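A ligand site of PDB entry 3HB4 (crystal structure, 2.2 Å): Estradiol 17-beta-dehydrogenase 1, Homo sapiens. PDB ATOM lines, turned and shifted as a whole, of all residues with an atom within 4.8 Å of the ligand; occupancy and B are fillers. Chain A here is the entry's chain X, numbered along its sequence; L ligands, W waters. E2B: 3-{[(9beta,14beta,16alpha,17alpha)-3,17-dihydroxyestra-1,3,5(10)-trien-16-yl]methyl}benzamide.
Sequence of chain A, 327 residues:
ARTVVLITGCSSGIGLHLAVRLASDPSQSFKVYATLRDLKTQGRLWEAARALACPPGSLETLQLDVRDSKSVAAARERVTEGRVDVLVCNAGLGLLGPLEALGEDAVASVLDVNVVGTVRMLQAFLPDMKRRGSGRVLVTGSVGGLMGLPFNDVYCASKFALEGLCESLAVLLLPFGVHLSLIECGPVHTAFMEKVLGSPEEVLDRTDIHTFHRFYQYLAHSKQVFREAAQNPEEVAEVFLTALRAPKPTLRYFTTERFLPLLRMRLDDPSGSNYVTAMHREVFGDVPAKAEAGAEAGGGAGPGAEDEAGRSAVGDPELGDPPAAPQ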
ATOM      1  N   GLY A  94     -20.437   9.585   1.896  1.00  0.00           N
ATOM      2  CA  GLY A  94     -19.625  10.786   1.658  1.00  0.00           C
ATOM      3  C   GLY A  94     -20.477  11.967   1.326  1.00  0.00           C
ATOM      4  O   GLY A  94     -21.598  11.817   0.926  1.00  0.00           O
ATOM      5  N   LEU A  95     -19.930  13.181   1.484  1.00  0.00           N
ATOM      6  CA  LEU A  95     -20.567  14.354   0.966  1.00  0.00           C
ATOM      7  C   LEU A  95     -19.541  15.445   0.807  1.00  0.00           C
ATOM      8  O   LEU A  95     -18.856  15.881   1.795  1.00  0.00           O
ATOM      9  CB  LEU A  95     -21.748  14.786   1.853  1.00  0.00           C
ATOM     10  CG  LEU A  95     -22.723  15.850   1.343  1.00  0.00           C
ATOM     11  CD1 LEU A  95     -23.550  15.367   0.135  1.00  0.00           C
ATOM     12  CD2 LEU A  95     -23.633  16.279   2.504  1.00  0.00           C
ATOM     13  N   SER A 142     -11.830   8.151  10.054  1.00  0.00           N
ATOM     14  CA  SER A 142     -11.166   8.863   8.970  1.00  0.00           C
ATOM     15  C   SER A 142     -10.303   9.929   9.646  1.00  0.00           C
ATOM     16  O   SER A 142     -10.492  10.258  10.804  1.00  0.00           O
ATOM     17  CB  SER A 142     -12.202   9.511   8.045  1.00  0.00           C
ATOM     18  OG  SER A 142     -11.639  10.607   7.329  1.00  0.00           O
ATOM     19  N   VAL A 143      -9.341  10.416   8.917  1.00  0.00           N
ATOM     20  CA  VAL A 143      -8.459  11.440   9.401  1.00  0.00           C
ATOM     21  C   VAL A 143      -9.320  12.729   9.301  1.00  0.00           C
ATOM     22  O   VAL A 143      -9.056  13.667   9.975  1.00  0.00           O
ATOM     23  CB  VAL A 143      -7.117  11.404   8.580  1.00  0.00           C
ATOM     24  CG1 VAL A 143      -6.347  12.775   8.574  1.00  0.00           C
ATOM     25  CG2 VAL A 143      -6.149  10.227   9.067  1.00  0.00           C
ATOM     26  N   GLY A 144     -10.357  12.714   8.462  1.00  0.00           N
ATOM     27  CA  GLY A 144     -11.393  13.798   8.435  1.00  0.00           C
ATOM     28  C   GLY A 144     -12.289  13.850   9.698  1.00  0.00           C
ATOM     29  O   GLY A 144     -12.994  14.828   9.907  1.00  0.00           O
ATOM     30  N   LEU A 149     -11.612  19.681   6.975  1.00  0.00           N
ATOM     31  CA  LEU A 149     -11.203  19.957   5.584  1.00  0.00           C
ATOM     32  C   LEU A 149     -12.226  20.834   4.796  1.00  0.00           C
ATOM     33  O   LEU A 149     -13.389  20.534   4.806  1.00  0.00           O
ATOM     34  CB  LEU A 149     -10.953  18.679   4.806  1.00  0.00           C
ATOM     35  CG  LEU A 149      -9.728  17.831   5.268  1.00  0.00           C
ATOM     36  CD1 LEU A 149      -9.897  16.413   4.877  1.00  0.00           C
ATOM     37  CD2 LEU A 149      -8.420  18.320   4.681  1.00  0.00           C
ATOM     38  N   ASN A 152     -15.528  19.641   3.062  1.00  0.00           N
ATOM     39  CA  ASN A 152     -15.889  18.339   3.654  1.00  0.00           C
ATOM     40  C   ASN A 152     -16.648  18.622   4.969  1.00  0.00           C
ATOM     41  O   ASN A 152     -16.650  17.831   5.873  1.00  0.00           O
ATOM     42  CB  ASN A 152     -14.626  17.517   3.928  1.00  0.00           C
ATOM     43  CG  ASN A 152     -13.930  17.030   2.637  1.00  0.00           C
ATOM     44  OD1 ASN A 152     -14.124  15.914   2.213  1.00  0.00           O
ATOM     45  ND2 ASN A 152     -13.179  17.899   2.010  1.00  0.00           N
ATOM     46  N   TYR A 155     -19.246  15.875   5.897  1.00  0.00           N
ATOM     47  CA  TYR A 155     -18.511  14.603   6.108  1.00  0.00           C
ATOM     48  C   TYR A 155     -17.660  14.627   7.395  1.00  0.00           C
ATOM     49  O   TYR A 155     -17.654  13.631   8.211  1.00  0.00           O
ATOM     50  CB  TYR A 155     -17.577  14.380   4.878  1.00  0.00           C
ATOM     51  CG  TYR A 155     -16.687  13.167   5.016  1.00  0.00           C
ATOM     52  CD1 TYR A 155     -17.179  11.894   4.788  1.00  0.00           C
ATOM     53  CD2 TYR A 155     -15.433  13.298   5.444  1.00  0.00           C
ATOM     54  CE1 TYR A 155     -16.383  10.752   5.010  1.00  0.00           C
ATOM     55  CE2 TYR A 155     -14.572  12.217   5.574  1.00  0.00           C
ATOM     56  CZ  TYR A 155     -15.057  10.940   5.358  1.00  0.00           C
ATOM     57  OH  TYR A 155     -14.210   9.851   5.566  1.00  0.00           O
ATOM     58  N   CYS A 185      -8.422   6.004   8.932  1.00  0.00           N
ATOM     59  CA  CYS A 185      -7.922   5.879   7.552  1.00  0.00           C
ATOM     60  C   CYS A 185      -7.581   7.223   6.999  1.00  0.00           C
ATOM     61  O   CYS A 185      -8.333   8.191   7.101  1.00  0.00           O
ATOM     62  CB  CYS A 185      -8.958   5.149   6.633  1.00  0.00           C
ATOM     63  SG  CYS A 185      -9.401   3.505   7.370  1.00  0.00           S
ATOM     64  N   GLY A 186      -6.427   7.291   6.367  1.00  0.00           N
ATOM     65  CA  GLY A 186      -6.158   8.369   5.395  1.00  0.00           C
ATOM     66  C   GLY A 186      -6.855   8.089   4.089  1.00  0.00           C
ATOM     67  O   GLY A 186      -7.823   7.348   4.041  1.00  0.00           O
ATOM     68  N   PRO A 187      -6.384   8.720   2.978  1.00  0.00           N
ATOM     69  CA  PRO A 187      -7.015   8.470   1.684  1.00  0.00           C
ATOM     70  C   PRO A 187      -6.839   6.971   1.385  1.00  0.00           C
ATOM     71  O   PRO A 187      -5.758   6.436   1.655  1.00  0.00           O
ATOM     72  CB  PRO A 187      -6.175   9.313   0.713  1.00  0.00           C
ATOM     73  CG  PRO A 187      -5.485  10.351   1.596  1.00  0.00           C
ATOM     74  CD  PRO A 187      -5.324   9.743   2.941  1.00  0.00           C
ATOM     75  N   PHE A 192     -14.065   6.191  -4.228  1.00  0.00           N
ATOM     76  CA  PHE A 192     -14.606   6.875  -3.047  1.00  0.00           C
ATOM     77  C   PHE A 192     -15.413   8.080  -3.427  1.00  0.00           C
ATOM     78  O   PHE A 192     -16.611   8.055  -3.471  1.00  0.00           O
ATOM     79  CB  PHE A 192     -13.458   7.384  -2.167  1.00  0.00           C
ATOM     80  CG  PHE A 192     -13.253   6.587  -0.929  1.00  0.00           C
ATOM     81  CD1 PHE A 192     -14.232   5.747  -0.457  1.00  0.00           C
ATOM     82  CD2 PHE A 192     -12.088   6.690  -0.224  1.00  0.00           C
ATOM     83  CE1 PHE A 192     -14.017   5.014   0.691  1.00  0.00           C
ATOM     84  CE2 PHE A 192     -11.878   5.953   0.908  1.00  0.00           C
ATOM     85  CZ  PHE A 192     -12.854   5.124   1.364  1.00  0.00           C
ATOM     86  N   MET A 193     -14.700   9.156  -3.629  1.00  0.00           N
ATOM     87  CA  MET A 193     -15.346  10.411  -3.972  1.00  0.00           C
ATOM     88  C   MET A 193     -16.124  10.422  -5.268  1.00  0.00           C
ATOM     89  O   MET A 193     -15.895  11.275  -6.114  1.00  0.00           O
ATOM     90  CB  MET A 193     -14.330  11.551  -4.059  1.00  0.00           C
ATOM     91  CG  MET A 193     -13.427  11.765  -2.858  1.00  0.00           C
ATOM     92  SD  MET A 193     -11.972  12.717  -3.242  1.00  0.00           S
ATOM     93  CE  MET A 193     -12.195  14.071  -2.109  1.00  0.00           C
ATOM     94  N   VAL A 196     -20.495  11.625  -4.741  1.00  0.00           N
ATOM     95  CA  VAL A 196     -20.547  12.335  -3.470  1.00  0.00           C
ATOM     96  C   VAL A 196     -20.607  13.854  -3.739  1.00  0.00           C
ATOM     97  O   VAL A 196     -20.823  14.657  -2.816  1.00  0.00           O
ATOM     98  CB  VAL A 196     -19.354  11.936  -2.525  1.00  0.00           C
ATOM     99  CG1 VAL A 196     -19.363  10.431  -2.184  1.00  0.00           C
ATOM    100  CG2 VAL A 196     -18.028  12.357  -3.133  1.00  0.00           C
ATOM    101  N   TYR A 218      -9.527  23.108  -4.278  1.00  0.00           N
ATOM    102  CA  TYR A 218      -9.495  22.007  -3.269  1.00  0.00           C
ATOM    103  C   TYR A 218      -9.473  20.625  -3.985  1.00  0.00           C
ATOM    104  O   TYR A 218      -8.685  19.751  -3.640  1.00  0.00           O
ATOM    105  CB  TYR A 218     -10.711  22.054  -2.260  1.00  0.00           C
ATOM    106  CG  TYR A 218     -10.752  20.751  -1.444  1.00  0.00           C
ATOM    107  CD1 TYR A 218      -9.882  20.531  -0.386  1.00  0.00           C
ATOM    108  CD2 TYR A 218     -11.620  19.708  -1.836  1.00  0.00           C
ATOM    109  CE1 TYR A 218      -9.900  19.265   0.310  1.00  0.00           C
ATOM    110  CE2 TYR A 218     -11.650  18.517  -1.201  1.00  0.00           C
ATOM    111  CZ  TYR A 218     -10.802  18.282  -0.133  1.00  0.00           C
ATOM    112  OH  TYR A 218     -10.914  17.025   0.459  1.00  0.00           O
ATOM    113  N   HIS A 221      -5.990  19.900  -5.419  1.00  0.00           N
ATOM    114  CA  HIS A 221      -5.144  19.462  -4.314  1.00  0.00           C
ATOM    115  C   HIS A 221      -5.458  18.083  -3.730  1.00  0.00           C
ATOM    116  O   HIS A 221      -4.576  17.320  -3.460  1.00  0.00           O
ATOM    117  CB  HIS A 221      -5.223  20.474  -3.228  1.00  0.00           C
ATOM    118  CG  HIS A 221      -4.415  20.131  -2.022  1.00  0.00           C
ATOM    119  ND1 HIS A 221      -4.998  19.688  -0.859  1.00  0.00           N
ATOM    120  CD2 HIS A 221      -3.088  20.219  -1.788  1.00  0.00           C
ATOM    121  CE1 HIS A 221      -4.066  19.526   0.053  1.00  0.00           C
ATOM    122  NE2 HIS A 221      -2.896  19.824  -0.479  1.00  0.00           N
ATOM    123  N   SER A 222      -6.720  17.764  -3.578  1.00  0.00           N
ATOM    124  CA  SER A 222      -7.181  16.449  -3.157  1.00  0.00           C
ATOM    125  C   SER A 222      -6.699  15.317  -4.116  1.00  0.00           C
ATOM    126  O   SER A 222      -6.125  14.311  -3.677  1.00  0.00           O
ATOM    127  CB  SER A 222      -8.704  16.498  -3.065  1.00  0.00           C
ATOM    128  OG  SER A 222      -9.242  15.225  -2.845  1.00  0.00           O
ATOM    129  N   VAL A 225      -3.015  14.858  -3.373  1.00  0.00           N
ATOM    130  CA  VAL A 225      -2.856  14.130  -2.093  1.00  0.00           C
ATOM    131  C   VAL A 225      -3.177  12.620  -2.245  1.00  0.00           C
ATOM    132  O   VAL A 225      -2.467  11.767  -1.712  1.00  0.00           O
ATOM    133  CB  VAL A 225      -3.724  14.793  -0.975  1.00  0.00           C
ATOM    134  CG1 VAL A 225      -3.906  13.882   0.231  1.00  0.00           C
ATOM    135  CG2 VAL A 225      -3.157  16.178  -0.609  1.00  0.00           C
ATOM    136  N   PHE A 226      -4.234  12.319  -2.987  1.00  0.00           N
ATOM    137  CA  PHE A 226      -4.636  10.945  -3.181  1.00  0.00           C
ATOM    138  C   PHE A 226      -3.592  10.202  -3.964  1.00  0.00           C
ATOM    139  O   PHE A 226      -3.280   9.051  -3.629  1.00  0.00           O
ATOM    140  CB  PHE A 226      -5.987  10.835  -3.869  1.00  0.00           C
ATOM    141  CG  PHE A 226      -7.112  10.563  -2.914  1.00  0.00           C
ATOM    142  CD1 PHE A 226      -7.630   9.268  -2.744  1.00  0.00           C
ATOM    143  CD2 PHE A 226      -7.610  11.591  -2.112  1.00  0.00           C
ATOM    144  CE1 PHE A 226      -8.696   9.011  -1.816  1.00  0.00           C
ATOM    145  CE2 PHE A 226      -8.674  11.345  -1.162  1.00  0.00           C
ATOM    146  CZ  PHE A 226      -9.213  10.070  -1.033  1.00  0.00           C
ATOM    147  N   PHE A 259      -0.302  11.756   8.787  1.00  0.00           N
ATOM    148  CA  PHE A 259      -0.995  12.980   9.069  1.00  0.00           C
ATOM    149  C   PHE A 259      -0.748  13.408  10.500  1.00  0.00           C
ATOM    150  O   PHE A 259      -1.225  14.466  10.947  1.00  0.00           O
ATOM    151  CB  PHE A 259      -2.479  12.863   8.714  1.00  0.00           C
ATOM    152  CG  PHE A 259      -2.721  12.532   7.255  1.00  0.00           C
ATOM    153  CD1 PHE A 259      -2.604  13.527   6.264  1.00  0.00           C
ATOM    154  CD2 PHE A 259      -2.941  11.207   6.846  1.00  0.00           C
ATOM    155  CE1 PHE A 259      -2.776  13.221   4.902  1.00  0.00           C
ATOM    156  CE2 PHE A 259      -3.089  10.887   5.480  1.00  0.00           C
ATOM    157  CZ  PHE A 259      -3.035  11.909   4.507  1.00  0.00           C
ATOM    158  N   LEU A 262       0.600  17.046  11.209  1.00  0.00           N
ATOM    159  CA  LEU A 262      -0.548  17.938  11.065  1.00  0.00           C
ATOM    160  C   LEU A 262      -1.532  17.903  12.217  1.00  0.00           C
ATOM    161  O   LEU A 262      -2.004  18.940  12.624  1.00  0.00           O
ATOM    162  CB  LEU A 262      -1.312  17.561   9.811  1.00  0.00           C
ATOM    163  CG  LEU A 262      -2.132  18.616   9.100  1.00  0.00           C
ATOM    164  CD1 LEU A 262      -1.419  19.949   9.155  1.00  0.00           C
ATOM    165  CD2 LEU A 262      -2.316  18.122   7.671  1.00  0.00           C
ATOM    166  N   MET A 279      -3.530  24.710   7.117  1.00  0.00           N
ATOM    167  CA  MET A 279      -4.387  24.031   6.149  1.00  0.00           C
ATOM    168  C   MET A 279      -4.839  24.954   5.014  1.00  0.00           C
ATOM    169  O   MET A 279      -4.924  24.509   3.835  1.00  0.00           O
ATOM    170  CB  MET A 279      -5.557  23.323   6.805  1.00  0.00           C
ATOM    171  CG  MET A 279      -6.412  22.453   5.858  1.00  0.00           C
ATOM    172  SD  MET A 279      -5.623  20.996   5.054  1.00  0.00           S
ATOM    173  CE  MET A 279      -4.654  20.400   6.372  1.00  0.00           C
ATOM    174  N   GLU A 282      -1.772  25.003   2.786  1.00  0.00           N
ATOM    175  CA  GLU A 282      -1.717  23.657   2.206  1.00  0.00           C
ATOM    176  C   GLU A 282      -2.689  23.451   1.047  1.00  0.00           C
ATOM    177  O   GLU A 282      -2.317  22.890   0.022  1.00  0.00           O
ATOM    178  CB  GLU A 282      -1.966  22.579   3.246  1.00  0.00           C
ATOM    179  CG  GLU A 282      -0.778  22.173   4.083  1.00  0.00           C
ATOM    180  CD  GLU A 282      -0.302  20.778   3.763  1.00  0.00           C
ATOM    181  OE1 GLU A 282       0.367  20.622   2.715  1.00  0.00           O
ATOM    182  OE2 GLU A 282      -0.633  19.850   4.567  1.00  0.00           O
ATOM    183  N   VAL A 283      -3.942  23.871   1.211  1.00  0.00           N
ATOM    184  CA  VAL A 283      -4.975  23.560   0.214  1.00  0.00           C
ATOM    185  C   VAL A 283      -5.002  24.568  -0.954  1.00  0.00           C
ATOM    186  O   VAL A 283      -5.235  24.220  -2.119  1.00  0.00           O
ATOM    187  CB  VAL A 283      -6.426  23.445   0.859  1.00  0.00           C
ATOM    188  CG1 VAL A 283      -7.508  23.262  -0.207  1.00  0.00           C
ATOM    189  CG2 VAL A 283      -6.501  22.296   1.859  1.00  0.00           C
HETATM  190  N30 E2B L   1     -16.742   7.850   0.055  1.00  0.00           N
HETATM  191  C9  E2B L   1      -8.315  14.013   2.460  1.00  0.00           C
HETATM  192  C10 E2B L   1      -7.041  13.936   3.270  1.00  0.00           C
HETATM  193  C15 E2B L   1      -9.066  12.679   2.611  1.00  0.00           C
HETATM  194  C8  E2B L   1      -8.049  14.497   1.015  1.00  0.00           C
HETATM  195  C14 E2B L   1      -9.302  12.146   4.052  1.00  0.00           C
HETATM  196  C11 E2B L   1      -6.280  15.204   3.148  1.00  0.00           C
HETATM  197  C13 E2B L   1      -7.951  12.025   4.782  1.00  0.00           C
HETATM  198  C16 E2B L   1     -10.476  12.641   2.066  1.00  0.00           C
HETATM  199  C28 E2B L   1     -16.176   8.376   1.161  1.00  0.00           C
HETATM  200  C25 E2B L   1     -16.154  11.028   0.695  1.00  0.00           C
HETATM  201  C6  E2B L   1      -6.554  16.209   2.050  1.00  0.00           C
HETATM  202  C12 E2B L   1      -7.231  13.391   4.737  1.00  0.00           C
HETATM  203  C17 E2B L   1     -10.945  11.253   2.481  1.00  0.00           C
HETATM  204  C18 E2B L   1     -10.029  10.879   3.662  1.00  0.00           C
HETATM  205  C20 E2B L   1     -10.276  13.080   4.854  1.00  0.00           C
HETATM  206  C24 E2B L   1     -15.580   9.823   1.225  1.00  0.00           C
HETATM  207  C1  E2B L   1      -5.249  15.473   4.075  1.00  0.00           C
HETATM  208  C26 E2B L   1     -15.582  12.328   0.833  1.00  0.00           C
HETATM  209  C21 E2B L   1     -12.421  11.286   2.850  1.00  0.00           C
HETATM  210  C23 E2B L   1     -14.346  10.015   1.873  1.00  0.00           C
HETATM  211  C27 E2B L   1     -14.348  12.422   1.496  1.00  0.00           C
HETATM  212  C7  E2B L   1      -7.669  15.989   1.001  1.00  0.00           C
HETATM  213  C3  E2B L   1      -4.699  17.585   2.963  1.00  0.00           C
HETATM  214  C22 E2B L   1     -13.695  11.274   1.986  1.00  0.00           C
HETATM  215  C5  E2B L   1      -5.742  17.376   2.015  1.00  0.00           C
HETATM  216  C2  E2B L   1      -4.465  16.625   3.971  1.00  0.00           C
HETATM  217  O4  E2B L   1      -3.904  18.734   2.924  1.00  0.00           O
HETATM  218  O29 E2B L   1     -16.179   7.665   2.189  1.00  0.00           O
HETATM  219  O19 E2B L   1     -10.736  10.257   4.739  1.00  0.00           O
HETATM  220  O   HOH W   1     -10.907   7.438   4.311  1.00  0.00           O
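O19 of the ligand is in hydrogen-bond range of OG of Ser 142, 2.8 Å away. The side-chain sulfur (SD) of Met 279 lies within hydrogen-bond range of an oxygen (O4) of the ligand (3.6 Å).
OG of Ser 142 is in hydrogen-bond range of OH of Tyr 155 (3.2 Å). The backbone NH (N) of Gly 144 sits at hydrogen-bond distance from the side-chain hydroxyl (OG) of Ser 142, 2.7 Å away. A ring nitrogen (NE2) of His 221 is in hydrogen-bond range of the backbone carbonyl oxygen (O) of Glu 282 (3.2 Å). OH of Tyr 218 lies within hydrogen-bond range of ND2 of Asn 152 (2.9 Å). N of Val 143 lies within hydrogen-bond range of O of Cys 185 (3.0 Å).
Gly 94 touches the ligand (CA to C25, 3.6 Å). CB of Val 143 touches C13 of the ligand, 3.9 Å away. Gly 144 touches the ligand (N to C20, 3.6 Å). Leu 149 touches the ligand (CD1 to C20, 3.4 Å). Asn 152 touches the ligand (OD1 to C27, 3.6 Å). Tyr 155 touches the ligand (OH to C21, 3.6 Å). Cys 185 touches the ligand (O to O19, 3.95 Å). CD of Pro 187 touches C13 of the ligand, 3.9 Å away. Phe 192 touches the ligand. Tyr 218 touches the ligand (OH to C7, 3.4 Å). CE1 of His 221 touches O4 of the ligand, at 3.0 Å. Val 225 touches the ligand (CG2 to C5, 3.9 Å). Phe 226 touches the ligand. Phe 259 touches the ligand. Glu 282 touches the ligand. Hydrophobic or aromatic side chains that line the ligand: Val 143, Leu 149, Tyr 155, Pro 187, Phe 192, His 221, Val 225, Phe 226, Phe 259 and Met 279. Of the 24 residues printed, 17 come within 4 Å of the ligand. Along chain A the residues within 4 Å of the ligand span positions 94 to 282.
Water W1 lies within hydrogen-bond range of O19 of the ligand (2.9 Å) and O of Gly 186 (3.1 Å).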
